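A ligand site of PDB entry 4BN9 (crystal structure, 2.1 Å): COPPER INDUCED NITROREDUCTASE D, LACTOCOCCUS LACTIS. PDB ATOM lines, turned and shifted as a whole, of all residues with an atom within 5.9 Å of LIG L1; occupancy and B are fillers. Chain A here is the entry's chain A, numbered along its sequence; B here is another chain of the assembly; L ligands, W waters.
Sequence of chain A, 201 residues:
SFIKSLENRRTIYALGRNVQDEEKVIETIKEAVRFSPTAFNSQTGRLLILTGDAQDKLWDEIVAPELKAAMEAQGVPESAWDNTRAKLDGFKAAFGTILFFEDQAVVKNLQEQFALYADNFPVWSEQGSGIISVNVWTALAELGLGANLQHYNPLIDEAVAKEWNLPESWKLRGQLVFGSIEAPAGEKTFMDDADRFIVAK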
ATOM      1  N   ARG A   9      17.107  -9.527  -3.641  1.00  0.00           N
ATOM      2  CA  ARG A   9      18.055  -8.894  -4.550  1.00  0.00           C
ATOM      3  C   ARG A   9      18.610  -7.634  -3.918  1.00  0.00           C
ATOM      4  O   ARG A   9      17.846  -6.737  -3.541  1.00  0.00           O
ATOM      5  CB  ARG A   9      17.416  -8.535  -5.887  1.00  0.00           C
ATOM      6  CG  ARG A   9      18.406  -7.935  -6.890  1.00  0.00           C
ATOM      7  CD  ARG A   9      17.819  -6.751  -7.641  1.00  0.00           C
ATOM      8  NE  ARG A   9      17.271  -5.736  -6.748  1.00  0.00           N
ATOM      9  CZ  ARG A   9      17.999  -4.803  -6.136  1.00  0.00           C
ATOM     10  NH1 ARG A   9      19.317  -4.736  -6.312  1.00  0.00           N
ATOM     11  NH2 ARG A   9      17.410  -3.931  -5.335  1.00  0.00           N
ATOM     12  N   ARG A  10      19.936  -7.562  -3.792  1.00  0.00           N
ATOM     13  CA  ARG A  10      20.597  -6.396  -3.205  1.00  0.00           C
ATOM     14  C   ARG A  10      21.915  -6.119  -3.917  1.00  0.00           C
ATOM     15  O   ARG A  10      22.441  -6.952  -4.664  1.00  0.00           O
ATOM     16  CB  ARG A  10      20.874  -6.633  -1.717  1.00  0.00           C
ATOM     17  CG  ARG A  10      19.632  -6.791  -0.839  1.00  0.00           C
ATOM     18  CD  ARG A  10      18.812  -5.517  -0.739  1.00  0.00           C
ATOM     19  NE  ARG A  10      19.628  -4.372  -0.346  1.00  0.00           N
ATOM     20  CZ  ARG A  10      20.015  -4.110   0.901  1.00  0.00           C
ATOM     21  NH1 ARG A  10      19.661  -4.903   1.898  1.00  0.00           N
ATOM     22  NH2 ARG A  10      20.767  -3.038   1.148  1.00  0.00           N
ATOM     23  N   THR A  11      22.458  -4.932  -3.678  1.00  0.00           N
ATOM     24  CA  THR A  11      23.775  -4.578  -4.210  1.00  0.00           C
ATOM     25  C   THR A  11      24.863  -5.201  -3.345  1.00  0.00           C
ATOM     26  O   THR A  11      25.010  -4.850  -2.177  1.00  0.00           O
ATOM     27  CB  THR A  11      23.937  -3.046  -4.285  1.00  0.00           C
ATOM     28  OG1 THR A  11      23.162  -2.540  -5.372  1.00  0.00           O
ATOM     29  CG2 THR A  11      25.400  -2.668  -4.483  1.00  0.00           C
ATOM     30  N   ILE A  12      25.628  -6.121  -3.931  1.00  0.00           N
ATOM     31  CA  ILE A  12      26.710  -6.794  -3.226  1.00  0.00           C
ATOM     32  C   ILE A  12      28.039  -6.452  -3.869  1.00  0.00           C
ATOM     33  O   ILE A  12      28.286  -6.811  -5.029  1.00  0.00           O
ATOM     34  CB  ILE A  12      26.534  -8.323  -3.250  1.00  0.00           C
ATOM     35  CG1 ILE A  12      25.173  -8.727  -2.681  1.00  0.00           C
ATOM     36  CG2 ILE A  12      27.665  -9.002  -2.474  1.00  0.00           C
ATOM     37  CD1 ILE A  12      24.990  -8.401  -1.215  1.00  0.00           C
ATOM     38  N   TYR A  13      28.899  -5.756  -3.131  1.00  0.00           N
ATOM     39  CA  TYR A  13      30.201  -5.327  -3.647  1.00  0.00           C
ATOM     40  C   TYR A  13      31.300  -6.362  -3.378  1.00  0.00           C
ATOM     41  O   TYR A  13      32.267  -6.451  -4.134  1.00  0.00           O
ATOM     42  CB  TYR A  13      30.612  -3.978  -3.052  1.00  0.00           C
ATOM     43  CG  TYR A  13      29.782  -2.821  -3.568  1.00  0.00           C
ATOM     44  CD1 TYR A  13      29.750  -2.522  -4.926  1.00  0.00           C
ATOM     45  CD2 TYR A  13      29.041  -2.022  -2.700  1.00  0.00           C
ATOM     46  CE1 TYR A  13      29.003  -1.463  -5.406  1.00  0.00           C
ATOM     47  CE2 TYR A  13      28.292  -0.971  -3.175  1.00  0.00           C
ATOM     48  CZ  TYR A  13      28.271  -0.684  -4.528  1.00  0.00           C
ATOM     49  OH  TYR A  13      27.522   0.367  -5.003  1.00  0.00           O
ATOM     50  N   PHE A  91      35.944  -5.658  -8.470  1.00  0.00           N
ATOM     51  CA  PHE A  91      35.171  -6.070  -9.627  1.00  0.00           C
ATOM     52  C   PHE A  91      35.833  -7.283 -10.282  1.00  0.00           C
ATOM     53  O   PHE A  91      35.178  -8.294 -10.522  1.00  0.00           O
ATOM     54  CB  PHE A  91      35.058  -4.922 -10.631  1.00  0.00           C
ATOM     55  CG  PHE A  91      34.333  -3.725 -10.089  1.00  0.00           C
ATOM     56  CD1 PHE A  91      33.309  -3.867  -9.165  1.00  0.00           C
ATOM     57  CD2 PHE A  91      34.675  -2.446 -10.507  1.00  0.00           C
ATOM     58  CE1 PHE A  91      32.647  -2.761  -8.662  1.00  0.00           C
ATOM     59  CE2 PHE A  91      34.005  -1.341 -10.010  1.00  0.00           C
ATOM     60  CZ  PHE A  91      32.992  -1.495  -9.081  1.00  0.00           C
ATOM     61  N   VAL A 134      17.530  -5.689 -14.167  1.00  0.00           N
ATOM     62  CA  VAL A 134      17.082  -6.053 -12.818  1.00  0.00           C
ATOM     63  C   VAL A 134      16.500  -7.459 -12.766  1.00  0.00           C
ATOM     64  O   VAL A 134      16.593  -8.123 -11.734  1.00  0.00           O
ATOM     65  CB  VAL A 134      16.054  -5.047 -12.231  1.00  0.00           C
ATOM     66  CG1 VAL A 134      16.686  -3.670 -12.093  1.00  0.00           C
ATOM     67  CG2 VAL A 134      14.786  -4.992 -13.076  1.00  0.00           C
ATOM     68  N   TRP A 137      19.549  -9.560 -12.536  1.00  0.00           N
ATOM     69  CA  TRP A 137      20.049  -9.282 -11.192  1.00  0.00           C
ATOM     70  C   TRP A 137      19.291 -10.102 -10.148  1.00  0.00           C
ATOM     71  O   TRP A 137      19.891 -10.790  -9.315  1.00  0.00           O
ATOM     72  CB  TRP A 137      19.891  -7.789 -10.912  1.00  0.00           C
ATOM     73  CG  TRP A 137      20.705  -7.234  -9.779  1.00  0.00           C
ATOM     74  CD1 TRP A 137      21.311  -7.925  -8.773  1.00  0.00           C
ATOM     75  CD2 TRP A 137      20.978  -5.854  -9.544  1.00  0.00           C
ATOM     76  NE1 TRP A 137      21.946  -7.061  -7.924  1.00  0.00           N
ATOM     77  CE2 TRP A 137      21.766  -5.782  -8.383  1.00  0.00           C
ATOM     78  CE3 TRP A 137      20.640  -4.669 -10.204  1.00  0.00           C
ATOM     79  CZ2 TRP A 137      22.212  -4.573  -7.861  1.00  0.00           C
ATOM     80  CZ3 TRP A 137      21.097  -3.471  -9.694  1.00  0.00           C
ATOM     81  CH2 TRP A 137      21.869  -3.433  -8.535  1.00  0.00           C
ATOM     82  N   ASN A 148      26.493  -6.364  -8.503  1.00  0.00           N
ATOM     83  CA  ASN A 148      26.360  -4.915  -8.475  1.00  0.00           C
ATOM     84  C   ASN A 148      26.440  -4.371  -9.894  1.00  0.00           C
ATOM     85  O   ASN A 148      27.085  -4.961 -10.761  1.00  0.00           O
ATOM     86  CB  ASN A 148      27.417  -4.274  -7.580  1.00  0.00           C
ATOM     87  CG  ASN A 148      28.833  -4.519  -8.077  1.00  0.00           C
ATOM     88  OD1 ASN A 148      29.327  -3.829  -8.962  1.00  0.00           O
ATOM     89  ND2 ASN A 148      29.513  -5.501  -7.483  1.00  0.00           N
ATOM     90  N   LEU A 149      25.779  -3.240 -10.124  1.00  0.00           N
ATOM     91  CA  LEU A 149      25.632  -2.694 -11.467  1.00  0.00           C
ATOM     92  C   LEU A 149      26.511  -1.458 -11.658  1.00  0.00           C
ATOM     93  O   LEU A 149      26.387  -0.477 -10.920  1.00  0.00           O
ATOM     94  CB  LEU A 149      24.162  -2.334 -11.722  1.00  0.00           C
ATOM     95  CG  LEU A 149      23.849  -1.699 -13.073  1.00  0.00           C
ATOM     96  CD1 LEU A 149      24.087  -2.670 -14.207  1.00  0.00           C
ATOM     97  CD2 LEU A 149      22.424  -1.175 -13.084  1.00  0.00           C
ATOM     98  N   GLN A 150      27.386  -1.512 -12.650  1.00  0.00           N
ATOM     99  CA  GLN A 150      28.327  -0.424 -12.914  1.00  0.00           C
ATOM    100  C   GLN A 150      28.045   0.241 -14.262  1.00  0.00           C
ATOM    101  O   GLN A 150      27.371  -0.340 -15.122  1.00  0.00           O
ATOM    102  CB  GLN A 150      29.768  -0.945 -12.891  1.00  0.00           C
ATOM    103  CG  GLN A 150      30.186  -1.493 -11.548  1.00  0.00           C
ATOM    104  CD  GLN A 150      29.862  -0.537 -10.417  1.00  0.00           C
ATOM    105  OE1 GLN A 150      30.156   0.649 -10.502  1.00  0.00           O
ATOM    106  NE2 GLN A 150      29.256  -1.048  -9.354  1.00  0.00           N
ATOM    107  N   HIS A 151      28.583   1.438 -14.434  1.00  0.00           N
ATOM    108  CA  HIS A 151      28.366   2.208 -15.664  1.00  0.00           C
ATOM    109  C   HIS A 151      29.643   2.891 -16.134  1.00  0.00           C
ATOM    110  O   HIS A 151      29.845   4.092 -15.907  1.00  0.00           O
ATOM    111  CB  HIS A 151      27.266   3.240 -15.436  1.00  0.00           C
ATOM    112  CG  HIS A 151      25.910   2.642 -15.251  1.00  0.00           C
ATOM    113  ND1 HIS A 151      25.412   2.309 -14.012  1.00  0.00           N
ATOM    114  CD2 HIS A 151      24.959   2.277 -16.142  1.00  0.00           C
ATOM    115  CE1 HIS A 151      24.210   1.786 -14.143  1.00  0.00           C
ATOM    116  NE2 HIS A 151      23.915   1.749 -15.436  1.00  0.00           N
ATOM    117  N   ALA A 185      24.946  -7.142   2.148  1.00  0.00           N
ATOM    118  CA  ALA A 185      24.605  -5.810   1.684  1.00  0.00           C
ATOM    119  C   ALA A 185      24.644  -4.844   2.858  1.00  0.00           C
ATOM    120  O   ALA A 185      24.442  -5.248   4.000  1.00  0.00           O
ATOM    121  CB  ALA A 185      23.239  -5.816   1.047  1.00  0.00           C
ATOM    122  N   LYS A 188      19.995   0.061   4.011  1.00  0.00           N
ATOM    123  CA  LYS A 188      19.294   0.858   3.015  1.00  0.00           C
ATOM    124  C   LYS A 188      18.017   1.471   3.599  1.00  0.00           C
ATOM    125  O   LYS A 188      17.308   0.827   4.384  1.00  0.00           O
ATOM    126  CB  LYS A 188      18.948   0.006   1.791  1.00  0.00           C
ATOM    127  CG  LYS A 188      18.232   0.777   0.689  1.00  0.00           C
ATOM    128  CD  LYS A 188      17.984  -0.072  -0.544  1.00  0.00           C
ATOM    129  CE  LYS A 188      17.132  -1.285  -0.247  1.00  0.00           C
ATOM    130  NZ  LYS A 188      16.681  -1.966  -1.497  1.00  0.00           N
ATOM    131  N   PHE B  35      10.854  -2.369  -3.129  1.00  0.00           N
ATOM    132  CA  PHE B  35      11.999  -3.267  -3.220  1.00  0.00           C
ATOM    133  C   PHE B  35      12.647  -3.267  -4.595  1.00  0.00           C
ATOM    134  O   PHE B  35      13.418  -4.165  -4.931  1.00  0.00           O
ATOM    135  CB  PHE B  35      11.570  -4.678  -2.817  1.00  0.00           C
ATOM    136  CG  PHE B  35      11.073  -4.766  -1.398  1.00  0.00           C
ATOM    137  CD1 PHE B  35      11.820  -4.237  -0.356  1.00  0.00           C
ATOM    138  CD2 PHE B  35       9.842  -5.337  -1.117  1.00  0.00           C
ATOM    139  CE1 PHE B  35      11.358  -4.309   0.949  1.00  0.00           C
ATOM    140  CE2 PHE B  35       9.380  -5.409   0.188  1.00  0.00           C
ATOM    141  CZ  PHE B  35      10.139  -4.891   1.219  1.00  0.00           C
ATOM    142  N   SER B  36      12.347  -2.240  -5.392  1.00  0.00           N
ATOM    143  CA  SER B  36      12.985  -2.064  -6.687  1.00  0.00           C
ATOM    144  C   SER B  36      14.189  -1.139  -6.551  1.00  0.00           C
ATOM    145  O   SER B  36      14.115  -0.134  -5.851  1.00  0.00           O
ATOM    146  CB  SER B  36      11.991  -1.474  -7.697  1.00  0.00           C
ATOM    147  OG  SER B  36      10.937  -2.389  -7.962  1.00  0.00           O
ATOM    148  N   PRO B  37      15.298  -1.481  -7.223  1.00  0.00           N
ATOM    149  CA  PRO B  37      16.512  -0.653  -7.122  1.00  0.00           C
ATOM    150  C   PRO B  37      16.441   0.592  -7.992  1.00  0.00           C
ATOM    151  O   PRO B  37      15.832   0.562  -9.066  1.00  0.00           O
ATOM    152  CB  PRO B  37      17.600  -1.598  -7.623  1.00  0.00           C
ATOM    153  CG  PRO B  37      16.901  -2.454  -8.623  1.00  0.00           C
ATOM    154  CD  PRO B  37      15.497  -2.647  -8.104  1.00  0.00           C
ATOM    155  N   THR B  38      17.070   1.670  -7.539  1.00  0.00           N
ATOM    156  CA  THR B  38      17.191   2.893  -8.320  1.00  0.00           C
ATOM    157  C   THR B  38      18.582   3.490  -8.122  1.00  0.00           C
ATOM    158  O   THR B  38      19.183   3.358  -7.059  1.00  0.00           O
ATOM    159  CB  THR B  38      16.136   3.932  -7.905  1.00  0.00           C
ATOM    160  OG1 THR B  38      16.158   4.125  -6.484  1.00  0.00           O
ATOM    161  CG2 THR B  38      14.746   3.497  -8.329  1.00  0.00           C
ATOM    162  N   ALA B  39      19.079   4.161  -9.153  1.00  0.00           N
ATOM    163  CA  ALA B  39      20.369   4.842  -9.078  1.00  0.00           C
ATOM    164  C   ALA B  39      20.450   5.696  -7.813  1.00  0.00           C
ATOM    165  O   ALA B  39      19.563   6.518  -7.554  1.00  0.00           O
ATOM    166  CB  ALA B  39      20.586   5.694 -10.311  1.00  0.00           C
ATOM    167  N   PHE B  40      21.503   5.502  -7.034  1.00  0.00           N
ATOM    168  CA  PHE B  40      21.741   6.283  -5.817  1.00  0.00           C
ATOM    169  C   PHE B  40      20.630   6.098  -4.788  1.00  0.00           C
ATOM    170  O   PHE B  40      20.513   6.893  -3.861  1.00  0.00           O
ATOM    171  CB  PHE B  40      21.882   7.769  -6.151  1.00  0.00           C
ATOM    172  CG  PHE B  40      23.263   8.163  -6.609  1.00  0.00           C
ATOM    173  CD1 PHE B  40      23.701   7.883  -7.888  1.00  0.00           C
ATOM    174  CD2 PHE B  40      24.115   8.834  -5.740  1.00  0.00           C
ATOM    175  CE1 PHE B  40      24.963   8.252  -8.304  1.00  0.00           C
ATOM    176  CE2 PHE B  40      25.388   9.212  -6.156  1.00  0.00           C
ATOM    177  CZ  PHE B  40      25.808   8.921  -7.441  1.00  0.00           C
ATOM    178  N   ASN B  41      19.826   5.050  -4.942  1.00  0.00           N
ATOM    179  CA  ASN B  41      18.662   4.854  -4.088  1.00  0.00           C
ATOM    180  C   ASN B  41      17.780   6.090  -4.096  1.00  0.00           C
ATOM    181  O   ASN B  41      17.182   6.455  -3.082  1.00  0.00           O
ATOM    182  CB  ASN B  41      19.100   4.539  -2.654  1.00  0.00           C
ATOM    183  CG  ASN B  41      17.959   3.977  -1.814  1.00  0.00           C
ATOM    184  OD1 ASN B  41      17.068   3.303  -2.320  1.00  0.00           O
ATOM    185  ND2 ASN B  41      17.986   4.266  -0.508  1.00  0.00           N
ATOM    186  N   TRP B 124      18.991   7.001 -16.002  1.00  0.00           N
ATOM    187  CA  TRP B 124      18.759   6.065 -14.908  1.00  0.00           C
ATOM    188  C   TRP B 124      17.320   6.171 -14.393  1.00  0.00           C
ATOM    189  O   TRP B 124      16.746   5.195 -13.923  1.00  0.00           O
ATOM    190  CB  TRP B 124      19.737   6.318 -13.759  1.00  0.00           C
ATOM    191  CG  TRP B 124      21.160   5.969 -14.089  1.00  0.00           C
ATOM    192  CD1 TRP B 124      21.593   5.064 -15.011  1.00  0.00           C
ATOM    193  CD2 TRP B 124      22.340   6.522 -13.493  1.00  0.00           C
ATOM    194  NE1 TRP B 124      22.965   5.011 -15.026  1.00  0.00           N
ATOM    195  CE2 TRP B 124      23.444   5.896 -14.098  1.00  0.00           C
ATOM    196  CE3 TRP B 124      22.561   7.482 -12.501  1.00  0.00           C
ATOM    197  CZ2 TRP B 124      24.756   6.206 -13.754  1.00  0.00           C
ATOM    198  CZ3 TRP B 124      23.871   7.784 -12.151  1.00  0.00           C
ATOM    199  CH2 TRP B 124      24.951   7.153 -12.775  1.00  0.00           C
ATOM    200  N   GLN B 127      15.176   4.254 -16.898  1.00  0.00           N
ATOM    201  CA  GLN B 127      15.368   2.835 -16.599  1.00  0.00           C
ATOM    202  C   GLN B 127      14.601   2.460 -15.333  1.00  0.00           C
ATOM    203  O   GLN B 127      14.007   1.379 -15.253  1.00  0.00           O
ATOM    204  CB  GLN B 127      16.857   2.516 -16.446  1.00  0.00           C
ATOM    205  CG  GLN B 127      17.658   2.697 -17.736  1.00  0.00           C
ATOM    206  CD  GLN B 127      19.151   2.523 -17.543  1.00  0.00           C
ATOM    207  OE1 GLN B 127      19.629   2.268 -16.440  1.00  0.00           O
ATOM    208  NE2 GLN B 127      19.903   2.663 -18.629  1.00  0.00           N
ATOM    209  N   GLY B 128      14.605   3.350 -14.357  1.00  0.00           N
ATOM    210  CA  GLY B 128      13.904   3.131 -13.101  1.00  0.00           C
ATOM    211  C   GLY B 128      12.406   2.944 -13.273  1.00  0.00           C
ATOM    212  O   GLY B 128      11.783   2.159 -12.560  1.00  0.00           O
ATOM    213  N   ILE B 131      11.806  -0.463 -14.606  1.00  0.00           N
ATOM    214  CA  ILE B 131      12.043  -1.401 -13.520  1.00  0.00           C
ATOM    215  C   ILE B 131      10.827  -1.570 -12.608  1.00  0.00           C
ATOM    216  O   ILE B 131      10.381  -2.697 -12.360  1.00  0.00           O
ATOM    217  CB  ILE B 131      13.248  -0.967 -12.677  1.00  0.00           C
ATOM    218  CG1 ILE B 131      14.550  -1.277 -13.424  1.00  0.00           C
ATOM    219  CG2 ILE B 131      13.247  -1.648 -11.306  1.00  0.00           C
ATOM    220  CD1 ILE B 131      15.756  -0.529 -12.912  1.00  0.00           C
HETATM  221  N1  LIG L   1      25.561   1.059  -8.081  1.00  0.00           N
HETATM  222  C1  LIG L   1      27.033   1.282  -8.347  1.00  0.00           C
HETATM  223  O1  LIG L   1      27.838   0.856  -7.584  1.00  0.00           O
HETATM  224  N2  LIG L   1      27.443   2.012  -9.515  1.00  0.00           N
HETATM  225  C2  LIG L   1      26.517   2.503 -10.403  1.00  0.00           C
HETATM  226  O2  LIG L   1      26.864   3.059 -11.393  1.00  0.00           O
HETATM  227  C3  LIG L   1      25.083   2.282 -10.136  1.00  0.00           C
HETATM  228  N3  LIG L   1      24.212   2.737 -10.939  1.00  0.00           N
HETATM  229  C4  LIG L   1      22.793   2.224 -10.842  1.00  0.00           C
HETATM  230  C5  LIG L   1      21.825   2.486 -11.996  1.00  0.00           C
HETATM  231  C6  LIG L   1      20.578   2.042 -11.926  1.00  0.00           C
HETATM  232  C7  LIG L   1      19.613   2.312 -13.085  1.00  0.00           C
HETATM  233  C8  LIG L   1      20.110   1.263 -10.688  1.00  0.00           C
HETATM  234  C9  LIG L   1      18.681   0.742 -10.627  1.00  0.00           C
HETATM  235  C10 LIG L   1      20.948   1.035  -9.690  1.00  0.00           C
HETATM  236  C11 LIG L   1      22.381   1.542  -9.752  1.00  0.00           C
HETATM  237  N4  LIG L   1      23.305   1.310  -8.666  1.00  0.00           N
HETATM  238  C12 LIG L   1      24.659   1.530  -8.912  1.00  0.00           C
HETATM  239  C13 LIG L   1      22.885   0.568  -7.482  1.00  0.00           C
HETATM  240  C14 LIG L   1      21.900   1.386  -6.636  1.00  0.00           C
HETATM  241  O3  LIG L   1      22.578   2.380  -5.927  1.00  0.00           O
HETATM  242  C15 LIG L   1      21.192   0.458  -5.644  1.00  0.00           C
HETATM  243  O4  LIG L   1      20.411  -0.484  -6.334  1.00  0.00           O
HETATM  244  C16 LIG L   1      20.301   1.272  -4.703  1.00  0.00           C
HETATM  245  O5  LIG L   1      21.106   2.033  -3.846  1.00  0.00           O
HETATM  246  C17 LIG L   1      19.451   0.331  -3.855  1.00  0.00           C
HETATM  247  O6  LIG L   1      20.298  -0.554  -3.186  1.00  0.00           O
HETATM  248  P1  LIG L   1      20.136  -2.167  -3.453  1.00  0.00           P
HETATM  249  O7  LIG L   1      18.740  -2.568  -3.302  1.00  0.00           O
HETATM  250  O8  LIG L   1      20.632  -2.503  -4.988  1.00  0.00           O
HETATM  251  O9  LIG L   1      21.047  -3.003  -2.369  1.00  0.00           O
HETATM  252  N1  LG2 L   2      26.980   5.807  -9.955  1.00  0.00           N
HETATM  253  C1  LG2 L   2      25.905   5.482  -9.230  1.00  0.00           C
HETATM  254  C2  LG2 L   2      26.076   4.918  -7.963  1.00  0.00           C
HETATM  255  C3  LG2 L   2      27.358   4.699  -7.471  1.00  0.00           C
HETATM  256  C4  LG2 L   2      28.456   5.056  -8.251  1.00  0.00           C
HETATM  257  C5  LG2 L   2      28.237   5.606  -9.503  1.00  0.00           C
HETATM  258  C6  LG2 L   2      24.886   4.549  -7.146  1.00  0.00           C
HETATM  259  O1  LG2 L   2      24.894   4.742  -5.905  1.00  0.00           O
HETATM  260  O2  LG2 L   2      23.873   4.045  -7.706  1.00  0.00           O
HETATM  261  O   HOH W   1      25.226  -1.941  -7.620  1.00  0.00           O
HETATM  262  O   HOH W   2      21.987  -1.566  -0.663  1.00  0.00           O
HETATM  263  O   HOH W   3      29.688   3.155 -12.207  1.00  0.00           O
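Water W2 bridges an oxygen (O9) of LIG L1 (2.4 Å) and the guanidinium group (NH2) of Arg 10 (2.6 Å).
Water W3 lies within hydrogen-bond range of an oxygen (O2) of LIG L1, the backbone NH of His 151 and the side-chain amide oxygen of Gln 150.
Water W1 lies within hydrogen-bond range of the backbone NH (N) of Leu 149 (2.9 Å), a nitrogen (N1) of LIG L1 (3.1 Å) and the side-chain hydroxyl (OG1) of Thr 11 (3.1 Å).
O3 of LIG L1 is in hydrogen-bond range of O2 of LG2 L2 (2.8 Å).
The side-chain amino group of Lys 188 is in salt-bridge range of an oxygen (O7) of LIG L1 (2.8 Å).
The backbone carbonyl oxygen (O) of Leu 149 lies close to a nitrogen (N2) of LIG L1.
The backbone NH (N) of Phe 40 of chain B lies within hydrogen-bond range of an oxygen (O2) of LG2 L2.
OH of Tyr 13 lies within hydrogen-bond range of O1 of LIG L1 (2.6 Å).
N of Thr 11 is in hydrogen-bond range of O9 of LIG L1 (2.7 Å).
N of Asn 41 of chain B lies close to O5 of LIG L1, at 3.5 Å.
The guanidinium group of Arg 10 lies within salt-bridge range of an oxygen (O9) of LIG L1, 2.8 Å away.
N of Phe 40 of chain B sits at hydrogen-bond distance from O3 of LIG L1 (3.5 Å).
An oxygen (O8) of LIG L1 sits at hydrogen-bond distance from the side-chain hydroxyl (OG1) of Thr 11 (2.6 Å).
NE2 of Gln 150 lies within hydrogen-bond range of O1 of LIG L1 (3.0 Å).
An oxygen (O7) of LIG L1 lies within salt-bridge range of the guanidinium group of Arg 9 (2.8 Å).
ND1 of His 151 sits at hydrogen-bond distance from O2 of LIG L1 (3.1 Å).
Merely in contact with LIG L1: Pro 37 of chain B (3.3 Å), Thr 38 of chain B (3.3 Å), Gln 127 of chain B (3.4 Å), Ala 39 of chain B (3.4 Å), Trp 137 (3.9 Å), Trp 124 of chain B (3.9 Å) and Ile 131 of chain B (3.9 Å).
Hydrophobic or aromatic side chains within 4 Å of LIG L1: Tyr 13, Trp 137, Leu 149, His 151, Pro 37 of chain B, Ala 39 of chain B, Trp 124 of chain B and Ile 131 of chain B.
17 residues have an atom within 4 Å of LIG L1: Arg 9, Arg 10, Thr 11, Tyr 13, Trp 137, Leu 149, Gln 150, His 151, Lys 188, Pro 37 of chain B, Thr 38 of chain B, Ala 39 of chain B, Phe 40 of chain B, Asn 41 of chain B, Trp 124 of chain B, Gln 127 of chain B and Ile 131 of chain B.
The nearest printed residue that does not touch LIG L1 is Ala 185 (4.9 Å).
A ring nitrogen (NE2) of His 151 lies within hydrogen-bond range of the indole nitrogen (NE1) of Trp 124 of chain B (3.4 Å).
The side-chain amide nitrogen (NE2) of Gln 150 is in hydrogen-bond range of the side-chain amide oxygen (OD1) of Asn 148 (2.8 Å).
O of Arg 10 is in hydrogen-bond range of NE1 of Trp 137, at 3.3 Å.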
